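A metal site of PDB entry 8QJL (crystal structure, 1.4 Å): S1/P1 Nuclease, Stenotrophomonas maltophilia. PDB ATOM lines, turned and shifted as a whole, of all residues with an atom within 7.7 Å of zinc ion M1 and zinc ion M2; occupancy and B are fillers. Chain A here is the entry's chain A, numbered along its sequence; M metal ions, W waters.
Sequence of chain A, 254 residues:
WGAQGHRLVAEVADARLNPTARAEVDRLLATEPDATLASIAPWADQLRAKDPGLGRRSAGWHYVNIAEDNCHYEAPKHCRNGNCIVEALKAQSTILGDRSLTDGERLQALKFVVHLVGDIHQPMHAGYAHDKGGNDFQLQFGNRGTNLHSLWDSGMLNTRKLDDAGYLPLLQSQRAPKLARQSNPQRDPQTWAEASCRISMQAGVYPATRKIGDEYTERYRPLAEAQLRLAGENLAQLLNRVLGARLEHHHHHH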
ATOM      1  N   TRP A   1      25.689  22.909  23.843  1.00  0.00           N
ATOM      2  CA  TRP A   1      24.748  22.171  22.973  1.00  0.00           C
ATOM      3  C   TRP A   1      24.129  23.145  21.965  1.00  0.00           C
ATOM      4  O   TRP A   1      24.078  24.351  22.207  1.00  0.00           O
ATOM      5  CB  TRP A   1      23.620  21.579  23.790  1.00  0.00           C
ATOM      6  CG  TRP A   1      24.066  20.724  24.925  1.00  0.00           C
ATOM      7  CD1 TRP A   1      24.109  21.110  26.235  1.00  0.00           C
ATOM      8  CD2 TRP A   1      24.537  19.371  24.887  1.00  0.00           C
ATOM      9  NE1 TRP A   1      24.563  20.082  27.017  1.00  0.00           N
ATOM     10  CE2 TRP A   1      24.798  19.002  26.219  1.00  0.00           C
ATOM     11  CE3 TRP A   1      24.755  18.439  23.873  1.00  0.00           C
ATOM     12  CZ2 TRP A   1      25.291  17.744  26.569  1.00  0.00           C
ATOM     13  CZ3 TRP A   1      25.232  17.190  24.230  1.00  0.00           C
ATOM     14  CH2 TRP A   1      25.489  16.843  25.551  1.00  0.00           C
ATOM     15  N   GLY A   2      23.625  22.590  20.880  1.00  0.00           N
ATOM     16  CA  GLY A   2      22.659  23.316  20.044  1.00  0.00           C
ATOM     17  C   GLY A   2      21.314  23.463  20.718  1.00  0.00           C
ATOM     18  O   GLY A   2      21.109  23.036  21.879  1.00  0.00           O
ATOM     19  N   ALA A   3      20.402  24.111  20.027  1.00  0.00           N
ATOM     20  CA  ALA A   3      19.143  24.553  20.641  1.00  0.00           C
ATOM     21  C   ALA A   3      18.352  23.350  21.122  1.00  0.00           C
ATOM     22  O   ALA A   3      17.830  23.400  22.241  1.00  0.00           O
ATOM     23  CB  ALA A   3      18.386  25.423  19.686  1.00  0.00           C
ATOM     24  N   GLY A   5      19.338  20.410  22.178  1.00  0.00           N
ATOM     25  CA  GLY A   5      19.918  19.914  23.419  1.00  0.00           C
ATOM     26  C   GLY A   5      19.559  20.804  24.596  1.00  0.00           C
ATOM     27  O   GLY A   5      19.164  20.273  25.657  1.00  0.00           O
ATOM     28  N   HIS A   6      19.625  22.123  24.430  1.00  0.00           N
ATOM     29  CA  HIS A   6      19.241  23.061  25.512  1.00  0.00           C
ATOM     30  C   HIS A   6      17.768  22.882  25.904  1.00  0.00           C
ATOM     31  O   HIS A   6      17.469  22.868  27.111  1.00  0.00           O
ATOM     32  CB  HIS A   6      19.557  24.492  25.137  1.00  0.00           C
ATOM     33  CG  HIS A   6      21.005  24.760  25.293  1.00  0.00           C
ATOM     34  ND1 HIS A   6      21.601  24.813  26.536  1.00  0.00           N
ATOM     35  CD2 HIS A   6      21.994  24.874  24.377  1.00  0.00           C
ATOM     36  CE1 HIS A   6      22.929  24.939  26.371  1.00  0.00           C
ATOM     37  NE2 HIS A   6      23.189  24.995  25.042  1.00  0.00           N
ATOM     38  N   ALA A  41      15.592  28.258  26.841  1.00  0.00           N
ATOM     39  CA  ALA A  41      16.850  27.507  27.063  1.00  0.00           C
ATOM     40  C   ALA A  41      17.920  27.864  26.027  1.00  0.00           C
ATOM     41  O   ALA A  41      19.104  27.911  26.393  1.00  0.00           O
ATOM     42  CB  ALA A  41      16.593  26.014  27.137  1.00  0.00           C
ATOM     43  N   PRO A  42      17.607  28.056  24.733  1.00  0.00           N
ATOM     44  CA  PRO A  42      18.608  28.476  23.738  1.00  0.00           C
ATOM     45  C   PRO A  42      18.948  29.955  23.704  1.00  0.00           C
ATOM     46  O   PRO A  42      19.871  30.346  22.975  1.00  0.00           O
ATOM     47  CB  PRO A  42      17.952  28.097  22.400  1.00  0.00           C
ATOM     48  CG  PRO A  42      16.871  27.119  22.759  1.00  0.00           C
ATOM     49  CD  PRO A  42      16.354  27.678  24.054  1.00  0.00           C
ATOM     50  N   ALA A  44      20.542  32.201  25.325  1.00  0.00           N
ATOM     51  CA  ALA A  44      21.893  32.754  25.552  1.00  0.00           C
ATOM     52  C   ALA A  44      22.779  32.565  24.318  1.00  0.00           C
ATOM     53  O   ALA A  44      23.808  33.269  24.218  1.00  0.00           O
ATOM     54  CB  ALA A  44      22.550  32.157  26.764  1.00  0.00           C
ATOM     55  N   ASP A  45      22.416  31.660  23.385  1.00  0.00           N
ATOM     56  CA  ASP A  45      23.191  31.483  22.136  1.00  0.00           C
ATOM     57  C   ASP A  45      22.663  32.350  20.995  1.00  0.00           C
ATOM     58  O   ASP A  45      23.279  32.334  19.905  1.00  0.00           O
ATOM     59  CB  ASP A  45      23.115  30.026  21.653  1.00  0.00           C
ATOM     60  CG  ASP A  45      24.024  29.024  22.362  1.00  0.00           C
ATOM     61  OD1 ASP A  45      24.914  29.463  23.149  1.00  0.00           O
ATOM     62  OD2 ASP A  45      23.787  27.777  22.143  1.00  0.00           O
ATOM     63  N   GLN A  46      21.538  33.040  21.202  1.00  0.00           N
ATOM     64  CA  GLN A  46      20.769  33.666  20.120  1.00  0.00           C
ATOM     65  C   GLN A  46      20.731  35.174  20.292  1.00  0.00           C
ATOM     66  O   GLN A  46      19.927  35.822  19.623  1.00  0.00           O
ATOM     67  CB  GLN A  46      19.360  33.056  20.097  1.00  0.00           C
ATOM     68  CG  GLN A  46      19.392  31.572  19.791  1.00  0.00           C
ATOM     69  CD  GLN A  46      18.064  30.871  19.677  1.00  0.00           C
ATOM     70  OE1 GLN A  46      17.027  31.381  20.109  1.00  0.00           O
ATOM     71  NE2 GLN A  46      18.095  29.670  19.122  1.00  0.00           N
ATOM     72  N   SER A  58      28.829  38.099  27.111  1.00  0.00           N
ATOM     73  CA  SER A  58      28.587  36.790  27.779  1.00  0.00           C
ATOM     74  C   SER A  58      29.042  35.578  26.955  1.00  0.00           C
ATOM     75  O   SER A  58      28.866  34.469  27.414  1.00  0.00           O
ATOM     76  CB  SER A  58      27.140  36.662  28.161  1.00  0.00           C
ATOM     77  OG  SER A  58      26.277  36.691  27.049  1.00  0.00           O
ATOM     78  N   ALA A  59      29.661  35.766  25.791  1.00  0.00           N
ATOM     79  CA  ALA A  59      30.015  34.624  24.924  1.00  0.00           C
ATOM     80  C   ALA A  59      30.995  33.665  25.625  1.00  0.00           C
ATOM     81  O   ALA A  59      30.868  32.419  25.485  1.00  0.00           O
ATOM     82  CB  ALA A  59      30.555  35.062  23.605  1.00  0.00           C
ATOM     83  N   TRP A  61      31.082  32.934  28.682  1.00  0.00           N
ATOM     84  CA  TRP A  61      30.438  32.279  29.854  1.00  0.00           C
ATOM     85  C   TRP A  61      30.013  30.848  29.503  1.00  0.00           C
ATOM     86  O   TRP A  61      29.597  30.150  30.399  1.00  0.00           O
ATOM     87  CB  TRP A  61      29.224  33.072  30.318  1.00  0.00           C
ATOM     88  CG  TRP A  61      29.485  34.468  30.737  1.00  0.00           C
ATOM     89  CD1 TRP A  61      30.669  35.165  30.809  1.00  0.00           C
ATOM     90  CD2 TRP A  61      28.477  35.353  31.238  1.00  0.00           C
ATOM     91  NE1 TRP A  61      30.455  36.412  31.307  1.00  0.00           N
ATOM     92  CE2 TRP A  61      29.121  36.583  31.538  1.00  0.00           C
ATOM     93  CE3 TRP A  61      27.097  35.239  31.438  1.00  0.00           C
ATOM     94  CZ2 TRP A  61      28.420  37.667  32.050  1.00  0.00           C
ATOM     95  CZ3 TRP A  61      26.408  36.331  31.908  1.00  0.00           C
ATOM     96  CH2 TRP A  61      27.060  37.523  32.221  1.00  0.00           C
ATOM     97  N   HIS A  62      30.060  30.447  28.220  1.00  0.00           N
ATOM     98  CA  HIS A  62      29.517  29.134  27.808  1.00  0.00           C
ATOM     99  C   HIS A  62      30.525  27.995  27.981  1.00  0.00           C
ATOM    100  O   HIS A  62      30.131  26.857  27.791  1.00  0.00           O
ATOM    101  CB  HIS A  62      28.991  29.189  26.376  1.00  0.00           C
ATOM    102  CG  HIS A  62      27.880  30.150  26.179  1.00  0.00           C
ATOM    103  ND1 HIS A  62      26.654  29.785  25.606  1.00  0.00           N
ATOM    104  CD2 HIS A  62      27.828  31.475  26.427  1.00  0.00           C
ATOM    105  CE1 HIS A  62      25.913  30.892  25.522  1.00  0.00           C
ATOM    106  NE2 HIS A  62      26.599  31.920  26.029  1.00  0.00           N
ATOM    107  N   TYR A  63      31.766  28.268  28.368  1.00  0.00           N
ATOM    108  CA  TYR A  63      32.781  27.197  28.405  1.00  0.00           C
ATOM    109  C   TYR A  63      33.873  27.535  29.400  1.00  0.00           C
ATOM    110  O   TYR A  63      33.925  28.642  29.963  1.00  0.00           O
ATOM    111  CB  TYR A  63      33.349  26.928  27.029  1.00  0.00           C
ATOM    112  CG  TYR A  63      33.958  28.128  26.386  1.00  0.00           C
ATOM    113  CD1 TYR A  63      33.179  29.015  25.647  1.00  0.00           C
ATOM    114  CD2 TYR A  63      35.304  28.408  26.573  1.00  0.00           C
ATOM    115  CE1 TYR A  63      33.759  30.152  25.110  1.00  0.00           C
ATOM    116  CE2 TYR A  63      35.900  29.532  26.005  1.00  0.00           C
ATOM    117  CZ  TYR A  63      35.125  30.398  25.276  1.00  0.00           C
ATOM    118  OH  TYR A  63      35.708  31.515  24.717  1.00  0.00           O
ATOM    119  N   ILE A  85      32.348  29.575  32.348  1.00  0.00           N
ATOM    120  CA  ILE A  85      31.033  29.030  32.746  1.00  0.00           C
ATOM    121  C   ILE A  85      30.983  28.788  34.248  1.00  0.00           C
ATOM    122  O   ILE A  85      29.885  28.838  34.797  1.00  0.00           O
ATOM    123  CB  ILE A  85      30.725  27.777  31.930  1.00  0.00           C
ATOM    124  CG1 ILE A  85      29.265  27.369  32.087  1.00  0.00           C
ATOM    125  CG2 ILE A  85      31.679  26.626  32.227  1.00  0.00           C
ATOM    126  CD1 ILE A  85      28.762  26.505  30.942  1.00  0.00           C
ATOM    127  N   HIS A 115      20.516  27.807  30.503  1.00  0.00           N
ATOM    128  CA  HIS A 115      21.434  27.534  29.403  1.00  0.00           C
ATOM    129  C   HIS A 115      22.725  26.929  29.936  1.00  0.00           C
ATOM    130  O   HIS A 115      23.250  25.965  29.370  1.00  0.00           O
ATOM    131  CB  HIS A 115      21.726  28.798  28.625  1.00  0.00           C
ATOM    132  CG  HIS A 115      22.474  28.538  27.370  1.00  0.00           C
ATOM    133  ND1 HIS A 115      21.815  28.254  26.184  1.00  0.00           N
ATOM    134  CD2 HIS A 115      23.802  28.545  27.108  1.00  0.00           C
ATOM    135  CE1 HIS A 115      22.739  28.072  25.234  1.00  0.00           C
ATOM    136  NE2 HIS A 115      23.979  28.253  25.777  1.00  0.00           N
ATOM    137  N   LEU A 116      23.296  27.575  30.937  1.00  0.00           N
ATOM    138  CA  LEU A 116      24.667  27.261  31.398  1.00  0.00           C
ATOM    139  C   LEU A 116      24.666  25.900  32.126  1.00  0.00           C
ATOM    140  O   LEU A 116      25.668  25.185  32.044  1.00  0.00           O
ATOM    141  CB  LEU A 116      25.217  28.380  32.275  1.00  0.00           C
ATOM    142  CG  LEU A 116      25.469  29.707  31.546  1.00  0.00           C
ATOM    143  CD1 LEU A 116      26.044  30.670  32.520  1.00  0.00           C
ATOM    144  CD2 LEU A 116      26.363  29.552  30.341  1.00  0.00           C
ATOM    145  N   GLY A 118      23.019  23.480  31.089  1.00  0.00           N
ATOM    146  CA  GLY A 118      23.159  22.639  29.882  1.00  0.00           C
ATOM    147  C   GLY A 118      24.614  22.612  29.384  1.00  0.00           C
ATOM    148  O   GLY A 118      25.222  21.547  29.300  1.00  0.00           O
ATOM    149  N   ASP A 119      25.189  23.789  29.130  1.00  0.00           N
ATOM    150  CA  ASP A 119      26.533  23.839  28.526  1.00  0.00           C
ATOM    151  C   ASP A 119      27.594  23.219  29.441  1.00  0.00           C
ATOM    152  O   ASP A 119      28.562  22.614  28.922  1.00  0.00           O
ATOM    153  CB  ASP A 119      26.960  25.251  28.151  1.00  0.00           C
ATOM    154  CG  ASP A 119      26.471  25.682  26.776  1.00  0.00           C
ATOM    155  OD1 ASP A 119      25.968  24.844  26.030  1.00  0.00           O
ATOM    156  OD2 ASP A 119      26.615  26.922  26.468  1.00  0.00           O
ATOM    157  N   ILE A 120      27.478  23.309  30.762  1.00  0.00           N
ATOM    158  CA  ILE A 120      28.546  22.836  31.663  1.00  0.00           C
ATOM    159  C   ILE A 120      28.547  21.314  31.715  1.00  0.00           C
ATOM    160  O   ILE A 120      29.503  20.760  32.234  1.00  0.00           O
ATOM    161  CB  ILE A 120      28.408  23.488  33.054  1.00  0.00           C
ATOM    162  CG1 ILE A 120      29.724  23.514  33.814  1.00  0.00           C
ATOM    163  CG2 ILE A 120      27.311  22.887  33.897  1.00  0.00           C
ATOM    164  CD1 ILE A 120      29.717  24.448  35.032  1.00  0.00           C
ATOM    165  N   GLN A 122      28.172  19.632  28.718  1.00  0.00           N
ATOM    166  CA  GLN A 122      28.633  19.249  27.363  1.00  0.00           C
ATOM    167  C   GLN A 122      30.133  19.061  27.490  1.00  0.00           C
ATOM    168  O   GLN A 122      30.843  20.055  27.692  1.00  0.00           O
ATOM    169  CB  GLN A 122      28.258  20.337  26.365  1.00  0.00           C
ATOM    170  CG  GLN A 122      28.056  19.908  24.914  1.00  0.00           C
ATOM    171  CD  GLN A 122      29.282  19.444  24.167  1.00  0.00           C
ATOM    172  OE1 GLN A 122      30.026  18.573  24.624  1.00  0.00           O
ATOM    173  NE2 GLN A 122      29.528  20.032  22.994  1.00  0.00           N
ATOM    174  N   HIS A 125      32.589  21.608  26.060  1.00  0.00           N
ATOM    175  CA  HIS A 125      32.539  22.948  26.667  1.00  0.00           C
ATOM    176  C   HIS A 125      33.462  23.022  27.895  1.00  0.00           C
ATOM    177  O   HIS A 125      33.527  24.134  28.482  1.00  0.00           O
ATOM    178  CB  HIS A 125      31.110  23.354  27.021  1.00  0.00           C
ATOM    179  CG  HIS A 125      30.310  23.840  25.858  1.00  0.00           C
ATOM    180  ND1 HIS A 125      29.797  25.110  25.823  1.00  0.00           N
ATOM    181  CD2 HIS A 125      30.006  23.249  24.652  1.00  0.00           C
ATOM    182  CE1 HIS A 125      29.192  25.289  24.646  1.00  0.00           C
ATOM    183  NE2 HIS A 125      29.340  24.179  23.888  1.00  0.00           N
ATOM    184  N   HIS A 149      33.773  19.387  18.424  1.00  0.00           N
ATOM    185  CA  HIS A 149      32.903  20.251  19.250  1.00  0.00           C
ATOM    186  C   HIS A 149      31.458  20.165  18.734  1.00  0.00           C
ATOM    187  O   HIS A 149      30.538  19.833  19.505  1.00  0.00           O
ATOM    188  CB  HIS A 149      33.411  21.681  19.273  1.00  0.00           C
ATOM    189  CG  HIS A 149      32.680  22.511  20.269  1.00  0.00           C
ATOM    190  ND1 HIS A 149      33.119  22.743  21.532  1.00  0.00           N
ATOM    191  CD2 HIS A 149      31.433  22.992  20.187  1.00  0.00           C
ATOM    192  CE1 HIS A 149      32.167  23.422  22.191  1.00  0.00           C
ATOM    193  NE2 HIS A 149      31.101  23.557  21.385  1.00  0.00           N
ATOM    194  N   ASP A 153      27.900  18.964  20.236  1.00  0.00           N
ATOM    195  CA  ASP A 153      26.835  19.969  20.409  1.00  0.00           C
ATOM    196  C   ASP A 153      25.538  19.488  19.771  1.00  0.00           C
ATOM    197  O   ASP A 153      24.463  19.755  20.363  1.00  0.00           O
ATOM    198  CB  ASP A 153      27.168  21.335  19.816  1.00  0.00           C
ATOM    199  CG  ASP A 153      27.865  22.334  20.738  1.00  0.00           C
ATOM    200  OD1 ASP A 153      27.938  22.109  21.951  1.00  0.00           O
ATOM    201  OD2 ASP A 153      28.392  23.333  20.180  1.00  0.00           O
HETATM  202 ZN    ZN M   1      25.887  28.048  24.906  1.00  0.00          ZN
HETATM  203 ZN    ZN M   2      25.011  24.906  24.185  1.00  0.00          ZN
HETATM  204 ZN    ZN M   3      29.182  24.302  21.802  1.00  0.00          ZN
HETATM  205  O   HOH W   1      27.300  25.212  21.927  1.00  0.00           O
HETATM  206  O   HOH W   2      25.697  26.606  23.580  1.00  0.00           O
HETATM  207  O   HOH W   3      27.951  28.236  23.475  1.00  0.00           O
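NE1 of Trp 1 lies within hydrogen-bond range of O of Gly 118. O of Ala 41 sits at hydrogen-bond distance from ND1 of His 115. ND1 of His 6 is in hydrogen-bond range of ND1 of His 115. ND1 of His 125 lies within hydrogen-bond range of O of His 62 (2.7 Å).
Along chain A the residues within 4 Å of zinc ion M1 span positions 45 to 119. The nearest printed residue that does not touch zinc ion M1 is His 6 (4.1 Å).
Zinc ion M1 is bound by water W2 (2.0 Å), a ring nitrogen (ND1) of His 62 (2.0 Å), the side-chain carboxylate of Asp 119 (2.1 Å), a ring nitrogen (NE2) of His 115 (2.1 Å), the side-chain carboxylate of Asp 45 (2.5 Å) and water W3 (2.5 Å). Zinc ion M1 has six donor atoms within binding distance.
Water W2 is bound to zinc ion M2, 1.9 Å away. Zinc ion M2 is bound by NE2 of His 6 (2.0 Å). OD1 of Asp 119 binds zinc ion M2. Zinc ion M2 is bound by N of Trp 1 (2.1 Å). O of Trp 1 binds zinc ion M2 (2.3 Å). Zinc ion M2 has five donor atoms within binding distance.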
